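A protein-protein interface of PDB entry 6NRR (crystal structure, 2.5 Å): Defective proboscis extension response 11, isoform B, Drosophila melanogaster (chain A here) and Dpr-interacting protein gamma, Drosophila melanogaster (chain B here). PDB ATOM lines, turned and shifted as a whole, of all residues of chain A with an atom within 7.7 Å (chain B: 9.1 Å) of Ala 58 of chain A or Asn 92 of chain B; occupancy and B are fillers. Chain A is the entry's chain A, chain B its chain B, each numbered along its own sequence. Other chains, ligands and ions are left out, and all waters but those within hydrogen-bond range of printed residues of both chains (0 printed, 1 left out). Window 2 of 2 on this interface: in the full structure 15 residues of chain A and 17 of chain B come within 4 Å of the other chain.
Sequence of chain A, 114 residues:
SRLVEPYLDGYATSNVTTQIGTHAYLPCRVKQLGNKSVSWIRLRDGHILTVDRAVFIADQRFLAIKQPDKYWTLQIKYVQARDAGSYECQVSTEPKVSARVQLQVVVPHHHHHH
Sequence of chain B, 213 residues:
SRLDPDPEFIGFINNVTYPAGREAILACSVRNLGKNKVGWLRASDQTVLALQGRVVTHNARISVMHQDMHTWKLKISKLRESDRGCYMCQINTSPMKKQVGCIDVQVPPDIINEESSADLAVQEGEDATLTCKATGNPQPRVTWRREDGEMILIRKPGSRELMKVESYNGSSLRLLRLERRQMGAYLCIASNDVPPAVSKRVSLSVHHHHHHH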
ATOM      1  N   HIS A  47      11.475  22.057 -24.712  1.00  0.00           N
ATOM      2  CA  HIS A  47      12.210  22.962 -23.840  1.00  0.00           C
ATOM      3  C   HIS A  47      12.968  24.001 -24.661  1.00  0.00           C
ATOM      4  O   HIS A  47      13.806  23.653 -25.496  1.00  0.00           O
ATOM      5  CB  HIS A  47      13.167  22.152 -22.959  1.00  0.00           C
ATOM      6  CG  HIS A  47      13.694  22.901 -21.773  1.00  0.00           C
ATOM      7  ND1 HIS A  47      14.093  24.221 -21.838  1.00  0.00           N
ATOM      8  CD2 HIS A  47      13.899  22.511 -20.494  1.00  0.00           C
ATOM      9  CE1 HIS A  47      14.510  24.612 -20.649  1.00  0.00           C
ATOM     10  NE2 HIS A  47      14.405  23.593 -19.816  1.00  0.00           N
ATOM     11  N   ILE A  48      12.664  25.279 -24.431  1.00  0.00           N
ATOM     12  CA  ILE A  48      13.447  26.348 -25.042  1.00  0.00           C
ATOM     13  C   ILE A  48      14.866  26.302 -24.491  1.00  0.00           C
ATOM     14  O   ILE A  48      15.082  26.241 -23.273  1.00  0.00           O
ATOM     15  CB  ILE A  48      12.794  27.715 -24.786  1.00  0.00           C
ATOM     16  CG1 ILE A  48      11.498  27.864 -25.586  1.00  0.00           C
ATOM     17  CG2 ILE A  48      13.752  28.845 -25.121  1.00  0.00           C
ATOM     18  CD1 ILE A  48      10.619  29.027 -25.136  1.00  0.00           C
ATOM     19  N   LEU A  49      15.848  26.312 -25.387  1.00  0.00           N
ATOM     20  CA  LEU A  49      17.246  26.226 -24.980  1.00  0.00           C
ATOM     21  C   LEU A  49      17.948  27.577 -25.060  1.00  0.00           C
ATOM     22  O   LEU A  49      18.444  28.088 -24.052  1.00  0.00           O
ATOM     23  CB  LEU A  49      17.984  25.195 -25.838  1.00  0.00           C
ATOM     24  CG  LEU A  49      17.367  23.803 -25.904  1.00  0.00           C
ATOM     25  CD1 LEU A  49      17.999  22.965 -27.020  1.00  0.00           C
ATOM     26  CD2 LEU A  49      17.491  23.096 -24.553  1.00  0.00           C
ATOM     27  N   VAL A  55      20.982  32.089 -23.164  1.00  0.00           N
ATOM     28  CA  VAL A  55      20.728  30.691 -22.837  1.00  0.00           C
ATOM     29  C   VAL A  55      19.586  30.645 -21.833  1.00  0.00           C
ATOM     30  O   VAL A  55      19.713  31.155 -20.717  1.00  0.00           O
ATOM     31  CB  VAL A  55      21.982  30.004 -22.276  1.00  0.00           C
ATOM     32  CG1 VAL A  55      21.710  28.535 -22.057  1.00  0.00           C
ATOM     33  CG2 VAL A  55      23.155  30.192 -23.217  1.00  0.00           C
ATOM     34  N   PHE A  56      18.472  30.028 -22.226  1.00  0.00           N
ATOM     35  CA  PHE A  56      17.300  29.958 -21.359  1.00  0.00           C
ATOM     36  C   PHE A  56      17.408  28.805 -20.372  1.00  0.00           C
ATOM     37  O   PHE A  56      17.141  28.972 -19.180  1.00  0.00           O
ATOM     38  CB  PHE A  56      16.040  29.822 -22.217  1.00  0.00           C
ATOM     39  CG  PHE A  56      14.761  29.712 -21.429  1.00  0.00           C
ATOM     40  CD1 PHE A  56      14.267  30.798 -20.724  1.00  0.00           C
ATOM     41  CD2 PHE A  56      14.036  28.529 -21.423  1.00  0.00           C
ATOM     42  CE1 PHE A  56      13.081  30.699 -20.012  1.00  0.00           C
ATOM     43  CE2 PHE A  56      12.857  28.420 -20.707  1.00  0.00           C
ATOM     44  CZ  PHE A  56      12.378  29.498 -20.006  1.00  0.00           C
ATOM     45  N   ILE A  57      17.802  27.629 -20.853  1.00  0.00           N
ATOM     46  CA  ILE A  57      17.839  26.448 -20.008  1.00  0.00           C
ATOM     47  C   ILE A  57      18.914  26.625 -18.943  1.00  0.00           C
ATOM     48  O   ILE A  57      19.957  27.252 -19.177  1.00  0.00           O
ATOM     49  CB  ILE A  57      18.081  25.197 -20.874  1.00  0.00           C
ATOM     50  CG1 ILE A  57      17.857  23.910 -20.076  1.00  0.00           C
ATOM     51  CG2 ILE A  57      19.475  25.236 -21.508  1.00  0.00           C
ATOM     52  CD1 ILE A  57      18.029  22.645 -20.902  1.00  0.00           C
ATOM     53  N   ALA A  58      18.649  26.098 -17.745  1.00  0.00           N
ATOM     54  CA  ALA A  58      19.565  26.336 -16.634  1.00  0.00           C
ATOM     55  C   ALA A  58      20.903  25.648 -16.861  1.00  0.00           C
ATOM     56  O   ALA A  58      21.941  26.163 -16.435  1.00  0.00           O
ATOM     57  CB  ALA A  58      18.938  25.877 -15.320  1.00  0.00           C
ATOM     58  N   ASP A  59      20.898  24.509 -17.544  1.00  0.00           N
ATOM     59  CA  ASP A  59      22.117  23.787 -17.891  1.00  0.00           C
ATOM     60  C   ASP A  59      23.086  24.646 -18.697  1.00  0.00           C
ATOM     61  O   ASP A  59      22.811  25.008 -19.847  1.00  0.00           O
ATOM     62  CB  ASP A  59      21.771  22.520 -18.677  1.00  0.00           C
ATOM     63  CG  ASP A  59      22.889  21.514 -18.659  1.00  0.00           C
ATOM     64  OD1 ASP A  59      24.047  21.907 -18.371  1.00  0.00           O
ATOM     65  OD2 ASP A  59      22.608  20.333 -18.935  1.00  0.00           O
ATOM     66  N   GLN A  60      24.238  24.949 -18.112  1.00  0.00           N
ATOM     67  CA  GLN A  60      25.202  25.854 -18.717  1.00  0.00           C
ATOM     68  C   GLN A  60      26.174  25.156 -19.650  1.00  0.00           C
ATOM     69  O   GLN A  60      27.090  25.802 -20.165  1.00  0.00           O
ATOM     70  CB  GLN A  60      25.973  26.606 -17.628  1.00  0.00           C
ATOM     71  CG  GLN A  60      25.179  27.717 -17.025  1.00  0.00           C
ATOM     72  CD  GLN A  60      26.059  28.749 -16.376  1.00  0.00           C
ATOM     73  OE1 GLN A  60      26.519  29.688 -17.029  1.00  0.00           O
ATOM     74  NE2 GLN A  60      26.305  28.585 -15.084  1.00  0.00           N
ATOM     75  N   ARG A  61      26.017  23.856 -19.858  1.00  0.00           N
ATOM     76  CA  ARG A  61      26.732  23.217 -20.949  1.00  0.00           C
ATOM     77  C   ARG A  61      26.201  23.653 -22.312  1.00  0.00           C
ATOM     78  O   ARG A  61      26.864  23.411 -23.326  1.00  0.00           O
ATOM     79  CB  ARG A  61      26.645  21.695 -20.803  1.00  0.00           C
ATOM     80  CG  ARG A  61      27.166  21.173 -19.470  1.00  0.00           C
ATOM     81  CD  ARG A  61      26.802  19.705 -19.275  1.00  0.00           C
ATOM     82  NE  ARG A  61      25.392  19.459 -19.575  1.00  0.00           N
ATOM     83  CZ  ARG A  61      24.952  18.600 -20.492  1.00  0.00           C
ATOM     84  NH1 ARG A  61      25.809  17.877 -21.198  1.00  0.00           N
ATOM     85  NH2 ARG A  61      23.652  18.454 -20.683  1.00  0.00           N
ATOM     86  N   PHE A  62      25.038  24.301 -22.356  1.00  0.00           N
ATOM     87  CA  PHE A  62      24.435  24.744 -23.606  1.00  0.00           C
ATOM     88  C   PHE A  62      24.910  26.148 -23.959  1.00  0.00           C
ATOM     89  O   PHE A  62      24.843  27.058 -23.129  1.00  0.00           O
ATOM     90  CB  PHE A  62      22.909  24.714 -23.504  1.00  0.00           C
ATOM     91  CG  PHE A  62      22.333  23.331 -23.548  1.00  0.00           C
ATOM     92  CD1 PHE A  62      22.251  22.562 -22.399  1.00  0.00           C
ATOM     93  CD2 PHE A  62      21.883  22.795 -24.741  1.00  0.00           C
ATOM     94  CE1 PHE A  62      21.725  21.282 -22.439  1.00  0.00           C
ATOM     95  CE2 PHE A  62      21.355  21.519 -24.785  1.00  0.00           C
ATOM     96  CZ  PHE A  62      21.277  20.762 -23.633  1.00  0.00           C
ATOM     97  N   ASP B   6      11.746  28.085  -4.850  1.00  0.00           N
ATOM     98  CA  ASP B   6      11.447  27.520  -6.160  1.00  0.00           C
ATOM     99  C   ASP B   6      10.193  28.169  -6.727  1.00  0.00           C
ATOM    100  O   ASP B   6       9.123  28.063  -6.118  1.00  0.00           O
ATOM    101  CB  ASP B   6      11.279  26.011  -6.076  1.00  0.00           C
ATOM    102  CG  ASP B   6      12.606  25.279  -6.170  1.00  0.00           C
ATOM    103  OD1 ASP B   6      13.406  25.626  -7.067  1.00  0.00           O
ATOM    104  OD2 ASP B   6      12.854  24.373  -5.340  1.00  0.00           O
ATOM    105  N   PRO B   7      10.278  28.853  -7.865  1.00  0.00           N
ATOM    106  CA  PRO B   7       9.085  29.501  -8.419  1.00  0.00           C
ATOM    107  C   PRO B   7       8.010  28.483  -8.763  1.00  0.00           C
ATOM    108  O   PRO B   7       8.292  27.332  -9.102  1.00  0.00           O
ATOM    109  CB  PRO B   7       9.610  30.215  -9.670  1.00  0.00           C
ATOM    110  CG  PRO B   7      10.902  29.562  -9.979  1.00  0.00           C
ATOM    111  CD  PRO B   7      11.474  29.090  -8.686  1.00  0.00           C
ATOM    112  N   PHE B   9       3.498  28.229 -10.063  1.00  0.00           N
ATOM    113  CA  PHE B   9       2.418  28.911 -10.756  1.00  0.00           C
ATOM    114  C   PHE B   9       1.310  29.265  -9.775  1.00  0.00           C
ATOM    115  O   PHE B   9       1.033  28.518  -8.833  1.00  0.00           O
ATOM    116  CB  PHE B   9       1.869  28.049 -11.899  1.00  0.00           C
ATOM    117  CG  PHE B   9       2.865  27.792 -13.007  1.00  0.00           C
ATOM    118  CD1 PHE B   9       3.180  28.786 -13.925  1.00  0.00           C
ATOM    119  CD2 PHE B   9       3.474  26.549 -13.142  1.00  0.00           C
ATOM    120  CE1 PHE B   9       4.086  28.549 -14.953  1.00  0.00           C
ATOM    121  CE2 PHE B   9       4.385  26.307 -14.166  1.00  0.00           C
ATOM    122  CZ  PHE B   9       4.692  27.307 -15.068  1.00  0.00           C
ATOM    123  N   VAL B  30       3.368  33.638 -11.873  1.00  0.00           N
ATOM    124  CA  VAL B  30       4.422  32.905 -11.181  1.00  0.00           C
ATOM    125  C   VAL B  30       4.792  33.645  -9.900  1.00  0.00           C
ATOM    126  O   VAL B  30       4.921  34.874  -9.891  1.00  0.00           O
ATOM    127  CB  VAL B  30       5.666  32.688 -12.084  1.00  0.00           C
ATOM    128  CG1 VAL B  30       5.261  32.172 -13.475  1.00  0.00           C
ATOM    129  CG2 VAL B  30       6.506  33.954 -12.217  1.00  0.00           C
ATOM    130  N   LEU B  33       9.602  34.089  -8.753  1.00  0.00           N
ATOM    131  CA  LEU B  33      10.365  33.810  -9.966  1.00  0.00           C
ATOM    132  C   LEU B  33      11.868  33.901  -9.716  1.00  0.00           C
ATOM    133  O   LEU B  33      12.644  33.139 -10.307  1.00  0.00           O
ATOM    134  CB  LEU B  33       9.957  34.769 -11.087  1.00  0.00           C
ATOM    135  CG  LEU B  33      10.620  34.511 -12.444  1.00  0.00           C
ATOM    136  CD1 LEU B  33      10.254  33.126 -12.971  1.00  0.00           C
ATOM    137  CD2 LEU B  33      10.257  35.593 -13.460  1.00  0.00           C
ATOM    138  N   GLY B  34      12.291  34.805  -8.833  1.00  0.00           N
ATOM    139  CA  GLY B  34      13.708  34.960  -8.557  1.00  0.00           C
ATOM    140  C   GLY B  34      14.482  35.273  -9.819  1.00  0.00           C
ATOM    141  O   GLY B  34      14.036  36.039 -10.681  1.00  0.00           O
ATOM    142  N   LYS B  35      15.658  34.658  -9.942  1.00  0.00           N
ATOM    143  CA  LYS B  35      16.502  34.861 -11.110  1.00  0.00           C
ATOM    144  C   LYS B  35      16.055  34.054 -12.323  1.00  0.00           C
ATOM    145  O   LYS B  35      16.631  34.227 -13.403  1.00  0.00           O
ATOM    146  CB  LYS B  35      17.952  34.520 -10.765  1.00  0.00           C
ATOM    147  CG  LYS B  35      18.648  35.553  -9.895  1.00  0.00           C
ATOM    148  CD  LYS B  35      18.854  36.859 -10.649  1.00  0.00           C
ATOM    149  CE  LYS B  35      19.857  37.761  -9.940  1.00  0.00           C
ATOM    150  NZ  LYS B  35      21.237  37.197  -9.970  1.00  0.00           N
ATOM    151  N   ASN B  36      15.046  33.198 -12.184  1.00  0.00           N
ATOM    152  CA  ASN B  36      14.569  32.398 -13.305  1.00  0.00           C
ATOM    153  C   ASN B  36      13.883  33.280 -14.348  1.00  0.00           C
ATOM    154  O   ASN B  36      13.722  34.491 -14.179  1.00  0.00           O
ATOM    155  CB  ASN B  36      13.617  31.306 -12.819  1.00  0.00           C
ATOM    156  CG  ASN B  36      14.323  30.234 -12.016  1.00  0.00           C
ATOM    157  OD1 ASN B  36      14.059  30.059 -10.826  1.00  0.00           O
ATOM    158  ND2 ASN B  36      15.229  29.511 -12.663  1.00  0.00           N
ATOM    159  N   LYS B  37      13.477  32.655 -15.451  1.00  0.00           N
ATOM    160  CA  LYS B  37      12.910  33.390 -16.573  1.00  0.00           C
ATOM    161  C   LYS B  37      11.713  32.638 -17.131  1.00  0.00           C
ATOM    162  O   LYS B  37      11.572  31.427 -16.947  1.00  0.00           O
ATOM    163  CB  LYS B  37      13.955  33.630 -17.668  1.00  0.00           C
ATOM    164  CG  LYS B  37      15.175  34.395 -17.169  1.00  0.00           C
ATOM    165  CD  LYS B  37      15.941  35.069 -18.291  1.00  0.00           C
ATOM    166  CE  LYS B  37      16.902  36.100 -17.720  1.00  0.00           C
ATOM    167  NZ  LYS B  37      17.828  35.500 -16.716  1.00  0.00           N
ATOM    168  N   VAL B  38      10.854  33.381 -17.828  1.00  0.00           N
ATOM    169  CA  VAL B  38       9.613  32.866 -18.403  1.00  0.00           C
ATOM    170  C   VAL B  38       9.672  33.005 -19.924  1.00  0.00           C
ATOM    171  O   VAL B  38       9.860  34.111 -20.449  1.00  0.00           O
ATOM    172  CB  VAL B  38       8.388  33.604 -17.841  1.00  0.00           C
ATOM    173  CG1 VAL B  38       7.116  33.119 -18.520  1.00  0.00           C
ATOM    174  CG2 VAL B  38       8.308  33.438 -16.326  1.00  0.00           C
ATOM    175  N   GLY B  39       9.493  31.893 -20.629  1.00  0.00           N
ATOM    176  CA  GLY B  39       9.427  31.901 -22.078  1.00  0.00           C
ATOM    177  C   GLY B  39       8.098  31.356 -22.571  1.00  0.00           C
ATOM    178  O   GLY B  39       7.432  30.583 -21.879  1.00  0.00           O
ATOM    179  N   LEU B  51      10.596  35.714 -24.862  1.00  0.00           N
ATOM    180  CA  LEU B  51      11.465  35.405 -23.739  1.00  0.00           C
ATOM    181  C   LEU B  51      11.476  36.622 -22.828  1.00  0.00           C
ATOM    182  O   LEU B  51      11.886  37.710 -23.251  1.00  0.00           O
ATOM    183  CB  LEU B  51      12.879  35.057 -24.215  1.00  0.00           C
ATOM    184  CG  LEU B  51      13.856  34.713 -23.102  1.00  0.00           C
ATOM    185  CD1 LEU B  51      13.201  33.723 -22.159  1.00  0.00           C
ATOM    186  CD2 LEU B  51      15.126  34.141 -23.686  1.00  0.00           C
ATOM    187  N   GLN B  52      11.007  36.437 -21.594  1.00  0.00           N
ATOM    188  CA  GLN B  52      10.873  37.521 -20.608  1.00  0.00           C
ATOM    189  C   GLN B  52       9.969  38.582 -21.230  1.00  0.00           C
ATOM    190  O   GLN B  52       8.939  38.222 -21.825  1.00  0.00           O
ATOM    191  CB  GLN B  52      12.249  38.006 -20.170  1.00  0.00           C
ATOM    192  CG  GLN B  52      12.966  37.051 -19.236  1.00  0.00           C
ATOM    193  CD  GLN B  52      12.212  36.834 -17.939  1.00  0.00           C
ATOM    194  OE1 GLN B  52      11.295  36.013 -17.863  1.00  0.00           O
ATOM    195  NE2 GLN B  52      12.595  37.572 -16.907  1.00  0.00           N
ATOM    196  N   CYS B  89       3.772  28.282 -21.442  1.00  0.00           N
ATOM    197  CA  CYS B  89       4.552  29.184 -20.605  1.00  0.00           C
ATOM    198  C   CYS B  89       5.584  28.344 -19.857  1.00  0.00           C
ATOM    199  O   CYS B  89       5.221  27.512 -19.024  1.00  0.00           O
ATOM    200  CB  CYS B  89       3.624  29.924 -19.646  1.00  0.00           C
ATOM    201  SG  CYS B  89       4.414  30.860 -18.343  1.00  0.00           S
ATOM    202  N   GLN B  90       6.863  28.550 -20.162  1.00  0.00           N
ATOM    203  CA  GLN B  90       7.952  27.753 -19.602  1.00  0.00           C
ATOM    204  C   GLN B  90       8.735  28.569 -18.580  1.00  0.00           C
ATOM    205  O   GLN B  90       9.113  29.714 -18.852  1.00  0.00           O
ATOM    206  CB  GLN B  90       8.910  27.270 -20.696  1.00  0.00           C
ATOM    207  CG  GLN B  90       8.268  26.487 -21.817  1.00  0.00           C
ATOM    208  CD  GLN B  90       9.284  25.928 -22.798  1.00  0.00           C
ATOM    209  OE1 GLN B  90      10.431  26.379 -22.859  1.00  0.00           O
ATOM    210  NE2 GLN B  90       8.867  24.931 -23.565  1.00  0.00           N
ATOM    211  N   ILE B  91       8.990  27.972 -17.418  1.00  0.00           N
ATOM    212  CA  ILE B  91       9.893  28.538 -16.423  1.00  0.00           C
ATOM    213  C   ILE B  91      11.179  27.734 -16.465  1.00  0.00           C
ATOM    214  O   ILE B  91      11.148  26.502 -16.359  1.00  0.00           O
ATOM    215  CB  ILE B  91       9.285  28.509 -15.009  1.00  0.00           C
ATOM    216  CG1 ILE B  91       7.955  29.262 -14.959  1.00  0.00           C
ATOM    217  CG2 ILE B  91      10.253  29.107 -14.007  1.00  0.00           C
ATOM    218  CD1 ILE B  91       7.249  29.126 -13.626  1.00  0.00           C
ATOM    219  N   ASN B  92      12.312  28.416 -16.610  1.00  0.00           N
ATOM    220  CA  ASN B  92      13.585  27.715 -16.765  1.00  0.00           C
ATOM    221  C   ASN B  92      14.140  27.168 -15.447  1.00  0.00           C
ATOM    222  O   ASN B  92      15.354  27.189 -15.210  1.00  0.00           O
ATOM    223  CB  ASN B  92      14.590  28.628 -17.461  1.00  0.00           C
ATOM    224  CG  ASN B  92      15.075  29.766 -16.590  1.00  0.00           C
ATOM    225  OD1 ASN B  92      14.477  30.099 -15.571  1.00  0.00           O
ATOM    226  ND2 ASN B  92      16.174  30.379 -17.001  1.00  0.00           N
ATOM    227  N   THR B  93      13.268  26.666 -14.576  1.00  0.00           N
ATOM    228  CA  THR B  93      13.717  25.851 -13.461  1.00  0.00           C
ATOM    229  C   THR B  93      14.270  24.523 -13.975  1.00  0.00           C
ATOM    230  O   THR B  93      14.094  24.151 -15.138  1.00  0.00           O
ATOM    231  CB  THR B  93      12.569  25.590 -12.490  1.00  0.00           C
ATOM    232  OG1 THR B  93      11.442  25.079 -13.215  1.00  0.00           O
ATOM    233  CG2 THR B  93      12.184  26.866 -11.794  1.00  0.00           C
ATOM    234  N   SER B  94      14.943  23.802 -13.091  1.00  0.00           N
ATOM    235  CA  SER B  94      15.469  22.482 -13.430  1.00  0.00           C
ATOM    236  C   SER B  94      14.914  21.458 -12.451  1.00  0.00           C
ATOM    237  O   SER B  94      15.230  21.526 -11.250  1.00  0.00           O
ATOM    238  CB  SER B  94      16.998  22.477 -13.415  1.00  0.00           C
ATOM    239  OG  SER B  94      17.500  21.328 -14.075  1.00  0.00           O
ATOM    240  N   PRO B  95      14.072  20.509 -12.891  1.00  0.00           N
ATOM    241  CA  PRO B  95      13.542  20.409 -14.257  1.00  0.00           C
ATOM    242  C   PRO B  95      12.600  21.549 -14.611  1.00  0.00           C
ATOM    243  O   PRO B  95      12.136  22.263 -13.728  1.00  0.00           O
ATOM    244  CB  PRO B  95      12.788  19.076 -14.248  1.00  0.00           C
ATOM    245  CG  PRO B  95      12.499  18.809 -12.805  1.00  0.00           C
ATOM    246  CD  PRO B  95      13.663  19.366 -12.059  1.00  0.00           C
ATOM    247  N   MET B  96      12.336  21.717 -15.900  1.00  0.00           N
ATOM    248  CA  MET B  96      11.505  22.820 -16.356  1.00  0.00           C
ATOM    249  C   MET B  96      10.089  22.698 -15.802  1.00  0.00           C
ATOM    250  O   MET B  96       9.567  21.596 -15.611  1.00  0.00           O
ATOM    251  CB  MET B  96      11.492  22.847 -17.885  1.00  0.00           C
ATOM    252  CG  MET B  96      10.536  23.839 -18.506  1.00  0.00           C
ATOM    253  SD  MET B  96      10.451  23.668 -20.296  1.00  0.00           S
ATOM    254  CE  MET B  96      10.463  21.877 -20.466  1.00  0.00           C
ATOM    255  N   LYS B  97       9.482  23.846 -15.510  1.00  0.00           N
ATOM    256  CA  LYS B  97       8.073  23.945 -15.168  1.00  0.00           C
ATOM    257  C   LYS B  97       7.331  24.619 -16.312  1.00  0.00           C
ATOM    258  O   LYS B  97       7.867  25.514 -16.976  1.00  0.00           O
ATOM    259  CB  LYS B  97       7.853  24.746 -13.877  1.00  0.00           C
ATOM    260  CG  LYS B  97       8.319  24.052 -12.601  1.00  0.00           C
ATOM    261  CD  LYS B  97       7.648  24.670 -11.383  1.00  0.00           C
ATOM    262  CE  LYS B  97       8.079  23.992 -10.095  1.00  0.00           C
ATOM    263  NZ  LYS B  97       9.002  24.854  -9.314  1.00  0.00           N
ATOM    264  N   LYS B  98       6.091  24.193 -16.539  1.00  0.00           N
ATOM    265  CA  LYS B  98       5.345  24.731 -17.665  1.00  0.00           C
ATOM    266  C   LYS B  98       3.855  24.707 -17.373  1.00  0.00           C
ATOM    267  O   LYS B  98       3.363  23.879 -16.603  1.00  0.00           O
ATOM    268  CB  LYS B  98       5.631  23.960 -18.959  1.00  0.00           C
ATOM    269  CG  LYS B  98       5.270  22.492 -18.886  1.00  0.00           C
ATOM    270  CD  LYS B  98       5.599  21.767 -20.181  1.00  0.00           C
ATOM    271  CE  LYS B  98       5.081  20.335 -20.164  1.00  0.00           C
ATOM    272  NZ  LYS B  98       5.743  19.511 -19.113  1.00  0.00           N
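Among the printed residues, pairs that only touch across the chains: His 47 of chain A with Gln 90 of chain B (3.9 Å), His 47 of chain A with Met 96 of chain B (3.5 Å), Phe 56 of chain A with Lys 37 of chain B (3.5 Å), Phe 56 of chain A with Gly 39 of chain B (3.8 Å), Phe 56 of chain A with Leu 51 of chain B (3.4 Å), Phe 56 of chain A with Gln 90 of chain B (3.5 Å) and Ala 58 of chain A with Asn 92 of chain B (3.8 Å).
N of Phe 56 of chain A lies within hydrogen-bond range of O of Leu 49 of chain A, 2.7 Å away. ND2 of Asn 36 of chain B lies within hydrogen-bond range of OD1 of Asn 92 of chain B. OD1 of Asn 92 of chain B sits at hydrogen-bond distance from N of Lys 37 of chain B (2.7 Å). The backbone carbonyl oxygen of Gly 39 of chain B is in hydrogen-bond range of the backbone NH of Gln 90 of chain B, at 2.7 Å. The side-chain amide oxygen of Gln 90 of chain B sits close to the side-chain sulfur of Met 96 of chain B (3.7 Å).
Printed residues of chain B within 4 Å of Ala 58 of chain A: Asn 92. Of the printed residues of chain A, Gly 39 of chain B touches Phe 56 (3.8 Å). Asn 92 of chain B touches two residues of chain A. Printed residues of chain A within 4 Å of Met 96 of chain B: His 47 (3.5 Å).
Printed residues of chain A that touch a printed residue of chain B: His 47, Ile 48, Phe 56 and Ala 58. Hydrophobic or aromatic side chains of chain A within 4 Å of the printed part of chain B: His 47, Ile 48, Phe 56 and Ala 58. Along chain A the printed residues that touch a printed residue of chain B span positions 47 to 58. Hydrophobic or aromatic side chains of chain B that line the printed part of chain A: Leu 51 and Met 96. Among the printed residues, 9 pairs touch across the chains.
OE1 of Gln 90 of chain B lies within hydrogen-bond range of N of Ile 48 of chain A (2.9 Å). ND2 of Asn 92 of chain B is in hydrogen-bond range of O of Phe 56 of chain A (2.8 Å).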
